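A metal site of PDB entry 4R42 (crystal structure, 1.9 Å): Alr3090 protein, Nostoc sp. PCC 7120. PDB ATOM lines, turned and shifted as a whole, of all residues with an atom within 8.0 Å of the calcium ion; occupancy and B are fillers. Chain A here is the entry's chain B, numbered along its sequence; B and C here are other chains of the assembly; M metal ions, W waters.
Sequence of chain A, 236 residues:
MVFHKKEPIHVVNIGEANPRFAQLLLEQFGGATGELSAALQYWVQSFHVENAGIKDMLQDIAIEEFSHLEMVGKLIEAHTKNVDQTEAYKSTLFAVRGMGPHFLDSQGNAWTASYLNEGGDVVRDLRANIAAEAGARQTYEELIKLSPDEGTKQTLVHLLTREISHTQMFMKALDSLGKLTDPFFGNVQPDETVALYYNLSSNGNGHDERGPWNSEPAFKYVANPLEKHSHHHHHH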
ATOM      1  N   ALA A  52      10.200  -2.393  15.148  1.00  0.00           N
ATOM      2  CA  ALA A  52      11.078  -3.561  15.247  1.00  0.00           C
ATOM      3  C   ALA A  52      10.434  -4.823  14.651  1.00  0.00           C
ATOM      4  O   ALA A  52      11.116  -5.659  14.051  1.00  0.00           O
ATOM      5  CB  ALA A  52      11.445  -3.814  16.698  1.00  0.00           C
ATOM      6  N   GLY A  53       9.132  -4.953  14.822  1.00  0.00           N
ATOM      7  CA  GLY A  53       8.405  -6.094  14.297  1.00  0.00           C
ATOM      8  C   GLY A  53       8.400  -6.102  12.773  1.00  0.00           C
ATOM      9  O   GLY A  53       8.647  -7.137  12.153  1.00  0.00           O
ATOM     10  N   LYS A  55      10.457  -4.363  10.834  1.00  0.00           N
ATOM     11  CA  LYS A  55      11.850  -4.490  10.402  1.00  0.00           C
ATOM     12  C   LYS A  55      12.220  -5.958  10.285  1.00  0.00           C
ATOM     13  O   LYS A  55      12.816  -6.405   9.295  1.00  0.00           O
ATOM     14  CB  LYS A  55      12.795  -3.774  11.369  1.00  0.00           C
ATOM     15  CG  LYS A  55      14.277  -3.926  11.015  1.00  0.00           C
ATOM     16  CD  LYS A  55      15.225  -3.248  12.017  1.00  0.00           C
ATOM     17  CE  LYS A  55      15.312  -1.731  11.830  1.00  0.00           C
ATOM     18  NZ  LYS A  55      16.719  -1.235  11.686  1.00  0.00           N
ATOM     19  N   ASP A  56      11.870  -6.714  11.319  1.00  0.00           N
ATOM     20  CA  ASP A  56      12.175  -8.135  11.369  1.00  0.00           C
ATOM     21  C   ASP A  56      11.452  -8.882  10.239  1.00  0.00           C
ATOM     22  O   ASP A  56      12.041  -9.728   9.558  1.00  0.00           O
ATOM     23  CB  ASP A  56      11.790  -8.734  12.722  1.00  0.00           C
ATOM     24  CG  ASP A  56      11.909 -10.230  12.756  1.00  0.00           C
ATOM     25  OD1 ASP A  56      13.018 -10.755  12.485  1.00  0.00           O
ATOM     26  OD2 ASP A  56      10.904 -10.901  13.025  1.00  0.00           O
ATOM     27  N   MET A  57      10.181  -8.542  10.027  1.00  0.00           N
ATOM     28  CA  MET A  57       9.395  -9.175   8.968  1.00  0.00           C
ATOM     29  C   MET A  57      10.059  -8.958   7.610  1.00  0.00           C
ATOM     30  O   MET A  57      10.149  -9.876   6.783  1.00  0.00           O
ATOM     31  CB  MET A  57       7.974  -8.607   8.963  1.00  0.00           C
ATOM     32  CG  MET A  57       7.053  -9.276   7.971  1.00  0.00           C
ATOM     33  SD  MET A  57       5.586  -8.298   7.563  1.00  0.00           S
ATOM     34  CE  MET A  57       6.363  -6.971   6.640  1.00  0.00           C
ATOM     35  N   LEU A  58      10.512  -7.740   7.383  1.00  0.00           N
ATOM     36  CA  LEU A  58      11.146  -7.414   6.119  1.00  0.00           C
ATOM     37  C   LEU A  58      12.394  -8.275   5.941  1.00  0.00           C
ATOM     38  O   LEU A  58      12.633  -8.801   4.851  1.00  0.00           O
ATOM     39  CB  LEU A  58      11.504  -5.942   6.071  1.00  0.00           C
ATOM     40  CG  LEU A  58      10.318  -5.001   5.944  1.00  0.00           C
ATOM     41  CD1 LEU A  58      10.776  -3.569   6.167  1.00  0.00           C
ATOM     42  CD2 LEU A  58       9.678  -5.129   4.555  1.00  0.00           C
ATOM     43  N   GLN A  59      13.162  -8.452   7.010  1.00  0.00           N
ATOM     44  CA  GLN A  59      14.363  -9.273   6.943  1.00  0.00           C
ATOM     45  C   GLN A  59      14.019 -10.749   6.758  1.00  0.00           C
ATOM     46  O   GLN A  59      14.685 -11.433   5.990  1.00  0.00           O
ATOM     47  CB  GLN A  59      15.233  -9.068   8.177  1.00  0.00           C
ATOM     48  CG  GLN A  59      15.798  -7.659   8.252  1.00  0.00           C
ATOM     49  CD  GLN A  59      16.497  -7.340   9.560  1.00  0.00           C
ATOM     50  OE1 GLN A  59      15.960  -7.587  10.644  1.00  0.00           O
ATOM     51  NE2 GLN A  59      17.692  -6.782   9.475  1.00  0.00           N
ATOM     52  N   ASP A  60      12.994 -11.237   7.446  1.00  0.00           N
ATOM     53  CA  ASP A  60      12.559 -12.639   7.294  1.00  0.00           C
ATOM     54  C   ASP A  60      12.207 -12.922   5.829  1.00  0.00           C
ATOM     55  O   ASP A  60      12.649 -13.915   5.248  1.00  0.00           O
ATOM     56  CB  ASP A  60      11.366 -12.955   8.204  1.00  0.00           C
ATOM     57  CG  ASP A  60      11.725 -13.105   9.677  1.00  0.00           C
ATOM     58  OD1 ASP A  60      12.879 -13.477   9.995  1.00  0.00           O
ATOM     59  OD2 ASP A  60      10.838 -12.890  10.532  1.00  0.00           O
ATOM     60  N   ILE A  61      11.421 -12.036   5.234  1.00  0.00           N
ATOM     61  CA  ILE A  61      10.962 -12.217   3.862  1.00  0.00           C
ATOM     62  C   ILE A  61      12.124 -12.039   2.873  1.00  0.00           C
ATOM     63  O   ILE A  61      12.265 -12.831   1.953  1.00  0.00           O
ATOM     64  CB  ILE A  61       9.823 -11.243   3.522  1.00  0.00           C
ATOM     65  CG1 ILE A  61       8.621 -11.530   4.432  1.00  0.00           C
ATOM     66  CG2 ILE A  61       9.389 -11.405   2.057  1.00  0.00           C
ATOM     67  CD1 ILE A  61       7.495 -10.509   4.308  1.00  0.00           C
ATOM     68  N   TYR B 197       4.949 -19.114   7.694  1.00  0.00           N
ATOM     69  CA  TYR B 197       5.884 -18.019   7.909  1.00  0.00           C
ATOM     70  C   TYR B 197       7.180 -18.604   8.413  1.00  0.00           C
ATOM     71  O   TYR B 197       7.194 -19.322   9.423  1.00  0.00           O
ATOM     72  CB  TYR B 197       5.330 -17.008   8.916  1.00  0.00           C
ATOM     73  CG  TYR B 197       6.192 -15.790   9.103  1.00  0.00           C
ATOM     74  CD1 TYR B 197       7.285 -15.803   9.954  1.00  0.00           C
ATOM     75  CD2 TYR B 197       5.907 -14.603   8.421  1.00  0.00           C
ATOM     76  CE1 TYR B 197       8.084 -14.672  10.133  1.00  0.00           C
ATOM     77  CE2 TYR B 197       6.694 -13.464   8.597  1.00  0.00           C
ATOM     78  CZ  TYR B 197       7.779 -13.506   9.456  1.00  0.00           C
ATOM     79  OH  TYR B 197       8.551 -12.373   9.648  1.00  0.00           O
ATOM     80  N   TYR B 198       8.277 -18.299   7.729  1.00  0.00           N
ATOM     81  CA  TYR B 198       9.588 -18.814   8.092  1.00  0.00           C
ATOM     82  C   TYR B 198      10.396 -17.748   8.823  1.00  0.00           C
ATOM     83  O   TYR B 198      10.654 -16.692   8.259  1.00  0.00           O
ATOM     84  CB  TYR B 198      10.368 -19.280   6.854  1.00  0.00           C
ATOM     85  CG  TYR B 198       9.657 -20.270   5.967  1.00  0.00           C
ATOM     86  CD1 TYR B 198       9.281 -21.523   6.437  1.00  0.00           C
ATOM     87  CD2 TYR B 198       9.373 -19.959   4.644  1.00  0.00           C
ATOM     88  CE1 TYR B 198       8.645 -22.441   5.609  1.00  0.00           C
ATOM     89  CE2 TYR B 198       8.736 -20.863   3.814  1.00  0.00           C
ATOM     90  CZ  TYR B 198       8.369 -22.093   4.301  1.00  0.00           C
ATOM     91  OH  TYR B 198       7.732 -22.983   3.470  1.00  0.00           O
ATOM     92  N   ASN B 199      10.792 -18.047  10.054  1.00  0.00           N
ATOM     93  CA  ASN B 199      11.628 -17.146  10.839  1.00  0.00           C
ATOM     94  C   ASN B 199      13.099 -17.236  10.405  1.00  0.00           C
ATOM     95  O   ASN B 199      13.919 -17.809  11.119  1.00  0.00           O
ATOM     96  CB  ASN B 199      11.489 -17.478  12.321  1.00  0.00           C
ATOM     97  CG  ASN B 199      12.273 -16.524  13.202  1.00  0.00           C
ATOM     98  OD1 ASN B 199      12.501 -15.375  12.828  1.00  0.00           O
ATOM     99  ND2 ASN B 199      12.684 -16.999  14.384  1.00  0.00           N
ATOM    100  N   LEU B 200      13.422 -16.658   9.255  1.00  0.00           N
ATOM    101  CA  LEU B 200      14.756 -16.837   8.675  1.00  0.00           C
ATOM    102  C   LEU B 200      15.789 -15.841   9.209  1.00  0.00           C
ATOM    103  O   LEU B 200      16.999 -16.075   9.108  1.00  0.00           O
ATOM    104  CB  LEU B 200      14.681 -16.746   7.156  1.00  0.00           C
ATOM    105  CG  LEU B 200      13.983 -17.955   6.532  1.00  0.00           C
ATOM    106  CD1 LEU B 200      13.562 -17.668   5.079  1.00  0.00           C
ATOM    107  CD2 LEU B 200      14.898 -19.172   6.573  1.00  0.00           C
ATOM    108  N   SER B 201      15.301 -14.730   9.774  1.00  0.00           N
ATOM    109  CA  SER B 201      16.156 -13.737  10.422  1.00  0.00           C
ATOM    110  C   SER B 201      15.819 -13.695  11.896  1.00  0.00           C
ATOM    111  O   SER B 201      14.699 -13.308  12.275  1.00  0.00           O
ATOM    112  CB  SER B 201      15.968 -12.351   9.790  1.00  0.00           C
ATOM    113  OG  SER B 201      16.811 -11.385  10.391  1.00  0.00           O
ATOM    114  N   SER B 202      16.769 -14.096  12.734  1.00  0.00           N
ATOM    115  CA  SER B 202      16.538 -14.243  14.167  1.00  0.00           C
ATOM    116  C   SER B 202      17.614 -13.563  14.992  1.00  0.00           C
ATOM    117  O   SER B 202      18.756 -13.388  14.537  1.00  0.00           O
ATOM    118  CB  SER B 202      16.455 -15.733  14.529  1.00  0.00           C
ATOM    119  OG  SER B 202      17.657 -16.407  14.186  1.00  0.00           O
ATOM    120  N   ASP B 208      12.629 -12.411  19.675  1.00  0.00           N
ATOM    121  CA  ASP B 208      11.931 -13.009  18.540  1.00  0.00           C
ATOM    122  C   ASP B 208      10.638 -12.237  18.241  1.00  0.00           C
ATOM    123  O   ASP B 208       9.647 -12.367  18.949  1.00  0.00           O
ATOM    124  CB  ASP B 208      11.620 -14.480  18.833  1.00  0.00           C
ATOM    125  CG  ASP B 208      11.526 -15.328  17.574  1.00  0.00           C
ATOM    126  OD1 ASP B 208      12.374 -15.158  16.669  1.00  0.00           O
ATOM    127  OD2 ASP B 208      10.605 -16.172  17.488  1.00  0.00           O
ATOM    128  N   GLU B 209      10.641 -11.440  17.166  1.00  0.00           N
ATOM    129  CA  GLU B 209       9.527 -10.535  16.909  1.00  0.00           C
ATOM    130  C   GLU B 209       8.331 -11.232  16.259  1.00  0.00           C
ATOM    131  O   GLU B 209       8.469 -11.967  15.279  1.00  0.00           O
ATOM    132  CB  GLU B 209       9.991  -9.361  16.039  1.00  0.00           C
ATOM    133  CG  GLU B 209      11.024  -8.457  16.701  1.00  0.00           C
ATOM    134  CD  GLU B 209      10.474  -7.615  17.852  1.00  0.00           C
ATOM    135  OE1 GLU B 209       9.252  -7.366  17.901  1.00  0.00           O
ATOM    136  OE2 GLU B 209      11.285  -7.184  18.695  1.00  0.00           O
ATOM    137  N   ARG B 210       7.165 -10.987  16.839  1.00  0.00           N
ATOM    138  CA  ARG B 210       5.915 -11.551  16.371  1.00  0.00           C
ATOM    139  C   ARG B 210       4.913 -10.432  16.099  1.00  0.00           C
ATOM    140  O   ARG B 210       4.950  -9.385  16.735  1.00  0.00           O
ATOM    141  CB  ARG B 210       5.323 -12.523  17.401  1.00  0.00           C
ATOM    142  CG  ARG B 210       6.237 -13.671  17.795  1.00  0.00           C
ATOM    143  CD  ARG B 210       6.563 -14.577  16.615  1.00  0.00           C
ATOM    144  NE  ARG B 210       5.378 -15.228  16.056  1.00  0.00           N
ATOM    145  CZ  ARG B 210       4.767 -16.277  16.595  1.00  0.00           C
ATOM    146  NH1 ARG B 210       5.218 -16.807  17.725  1.00  0.00           N
ATOM    147  NH2 ARG B 210       3.693 -16.803  16.001  1.00  0.00           N
ATOM    148  N   TRP B 213       1.421 -10.664  11.011  1.00  0.00           N
ATOM    149  CA  TRP B 213       2.047 -11.185   9.804  1.00  0.00           C
ATOM    150  C   TRP B 213       2.721 -12.543  10.004  1.00  0.00           C
ATOM    151  O   TRP B 213       3.138 -13.162   9.022  1.00  0.00           O
ATOM    152  CB  TRP B 213       3.090 -10.188   9.275  1.00  0.00           C
ATOM    153  CG  TRP B 213       4.086  -9.802  10.336  1.00  0.00           C
ATOM    154  CD1 TRP B 213       5.203 -10.494  10.724  1.00  0.00           C
ATOM    155  CD2 TRP B 213       4.032  -8.634  11.172  1.00  0.00           C
ATOM    156  NE1 TRP B 213       5.841  -9.831  11.746  1.00  0.00           N
ATOM    157  CE2 TRP B 213       5.140  -8.688  12.037  1.00  0.00           C
ATOM    158  CE3 TRP B 213       3.144  -7.557  11.275  1.00  0.00           C
ATOM    159  CZ2 TRP B 213       5.404  -7.690  12.981  1.00  0.00           C
ATOM    160  CZ3 TRP B 213       3.405  -6.566  12.214  1.00  0.00           C
ATOM    161  CH2 TRP B 213       4.520  -6.638  13.046  1.00  0.00           C
ATOM    162  N   ASN B 214       2.887 -12.985  11.249  1.00  0.00           N
ATOM    163  CA  ASN B 214       3.473 -14.313  11.471  1.00  0.00           C
ATOM    164  C   ASN B 214       2.847 -15.055  12.646  1.00  0.00           C
ATOM    165  O   ASN B 214       3.499 -15.890  13.258  1.00  0.00           O
ATOM    166  CB  ASN B 214       4.999 -14.211  11.670  1.00  0.00           C
ATOM    167  CG  ASN B 214       5.407 -13.406  12.899  1.00  0.00           C
ATOM    168  OD1 ASN B 214       4.642 -13.207  13.855  1.00  0.00           O
ATOM    169  ND2 ASN B 214       6.662 -12.974  12.887  1.00  0.00           N
ATOM    170  N   TYR B 221       3.530 -20.366  12.187  1.00  0.00           N
ATOM    171  CA  TYR B 221       4.878 -19.835  12.417  1.00  0.00           C
ATOM    172  C   TYR B 221       5.925 -20.951  12.519  1.00  0.00           C
ATOM    173  O   TYR B 221       5.789 -21.863  13.340  1.00  0.00           O
ATOM    174  CB  TYR B 221       4.870 -19.001  13.695  1.00  0.00           C
ATOM    175  CG  TYR B 221       6.146 -18.257  13.989  1.00  0.00           C
ATOM    176  CD1 TYR B 221       6.594 -17.251  13.146  1.00  0.00           C
ATOM    177  CD2 TYR B 221       6.890 -18.533  15.134  1.00  0.00           C
ATOM    178  CE1 TYR B 221       7.769 -16.554  13.415  1.00  0.00           C
ATOM    179  CE2 TYR B 221       8.058 -17.842  15.414  1.00  0.00           C
ATOM    180  CZ  TYR B 221       8.486 -16.853  14.552  1.00  0.00           C
ATOM    181  OH  TYR B 221       9.637 -16.156  14.816  1.00  0.00           O
ATOM    182  N   VAL B 222       6.953 -20.871  11.682  1.00  0.00           N
ATOM    183  CA  VAL B 222       8.058 -21.815  11.729  1.00  0.00           C
ATOM    184  C   VAL B 222       9.254 -21.131  12.381  1.00  0.00           C
ATOM    185  O   VAL B 222       9.987 -20.393  11.728  1.00  0.00           O
ATOM    186  CB  VAL B 222       8.439 -22.332  10.321  1.00  0.00           C
ATOM    187  CG1 VAL B 222       9.586 -23.337  10.395  1.00  0.00           C
ATOM    188  CG2 VAL B 222       7.231 -22.949   9.636  1.00  0.00           C
ATOM    189  N   ALA B 223       9.447 -21.383  13.668  1.00  0.00           N
ATOM    190  CA  ALA B 223      10.354 -20.571  14.470  1.00  0.00           C
ATOM    191  C   ALA B 223      11.816 -20.866  14.182  1.00  0.00           C
ATOM    192  O   ALA B 223      12.667 -19.982  14.303  1.00  0.00           O
ATOM    193  CB  ALA B 223      10.053 -20.764  15.948  1.00  0.00           C
ATOM    194  N   HIS C   4      20.097 -15.508   8.299  1.00  0.00           N
ATOM    195  CA  HIS C   4      20.569 -14.221   8.807  1.00  0.00           C
ATOM    196  C   HIS C   4      20.476 -14.150  10.330  1.00  0.00           C
ATOM    197  O   HIS C   4      19.431 -14.466  10.913  1.00  0.00           O
ATOM    198  CB  HIS C   4      19.775 -13.070   8.170  1.00  0.00           C
ATOM    199  CG  HIS C   4      20.262 -11.701   8.536  1.00  0.00           C
ATOM    200  ND1 HIS C   4      19.519 -10.824   9.309  1.00  0.00           N
ATOM    201  CD2 HIS C   4      21.397 -11.042   8.216  1.00  0.00           C
ATOM    202  CE1 HIS C   4      20.192  -9.698   9.453  1.00  0.00           C
ATOM    203  NE2 HIS C   4      21.333  -9.809   8.806  1.00  0.00           N
ATOM    204  N   LYS C   6      20.998 -11.261  13.377  1.00  0.00           N
ATOM    205  CA  LYS C   6      20.771  -9.827  13.306  1.00  0.00           C
ATOM    206  C   LYS C   6      21.951  -8.955  13.739  1.00  0.00           C
ATOM    207  O   LYS C   6      21.992  -7.768  13.408  1.00  0.00           O
ATOM    208  CB  LYS C   6      19.536  -9.490  14.135  1.00  0.00           C
ATOM    209  CG  LYS C   6      18.275 -10.078  13.525  1.00  0.00           C
ATOM    210  CD  LYS C   6      17.031  -9.792  14.340  1.00  0.00           C
ATOM    211  CE  LYS C   6      15.799 -10.353  13.644  1.00  0.00           C
ATOM    212  NZ  LYS C   6      15.605  -9.776  12.279  1.00  0.00           N
HETATM  213 CA    CA M   1      12.264 -13.075  12.488  1.00  0.00          CA
HETATM  214  O   HOH W   1      13.071 -12.813  14.927  1.00  0.00           O
HETATM  215  O   HOH W   2      10.136 -13.686  13.449  1.00  0.00           O
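Within 4 Å of the calcium ion: Asp 56, Asp 60, Asn 199 of chain B and Ser 201 of chain B.
Along chain A the residues within 4 Å of the calcium ion span positions 56 to 60.
The nearest printed residue that does not touch the calcium ion is Lys 6 of chain C (4.6 Å).
Water W2 lies within hydrogen-bond range of the side-chain hydroxyl (OH) of Tyr 221 of chain B and the backbone carbonyl oxygen (O) of Glu 209 of chain B.
ND2 of Asn 199 of chain B lies close to OH of Tyr 221 of chain B (3.2 Å).
ND2 of Asn 199 of chain B sits at hydrogen-bond distance from OD1 of Asp 208 of chain B (3.0 Å).
ND2 of Asn 199 of chain B is in hydrogen-bond range of O of Ala 223 of chain B (3.0 Å).
N of Asn 199 of chain B sits at hydrogen-bond distance from O of Val 222 of chain B (3.0 Å).
OH of Tyr 197 of chain B sits close to OD2 of Asp 60 (2.5 Å).
The side-chain carboxylate (OD1) of Asp 56 sits close to the side-chain amino group (NZ) of Lys 6 of chain C.
NZ of Lys 6 of chain C is in hydrogen-bond range of OG of Ser 201 of chain B (2.8 Å).
The side-chain hydroxyl of Ser 201 of chain B lies within hydrogen-bond range of a ring nitrogen (ND1) of His 4 of chain C (3.0 Å).
The calcium ion is bound by OD1 of Asn 199 of chain B (2.3 Å), water W2 (2.4 Å), OD2 of Asp 60 (2.4 Å), OD1 of Asp 56 (2.4 Å), O of Ser 201 of chain B (2.5 Å), water W1 (2.6 Å), OD1 of Asp 60 (2.6 Å) and OD2 of Asp 56 (2.6 Å).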
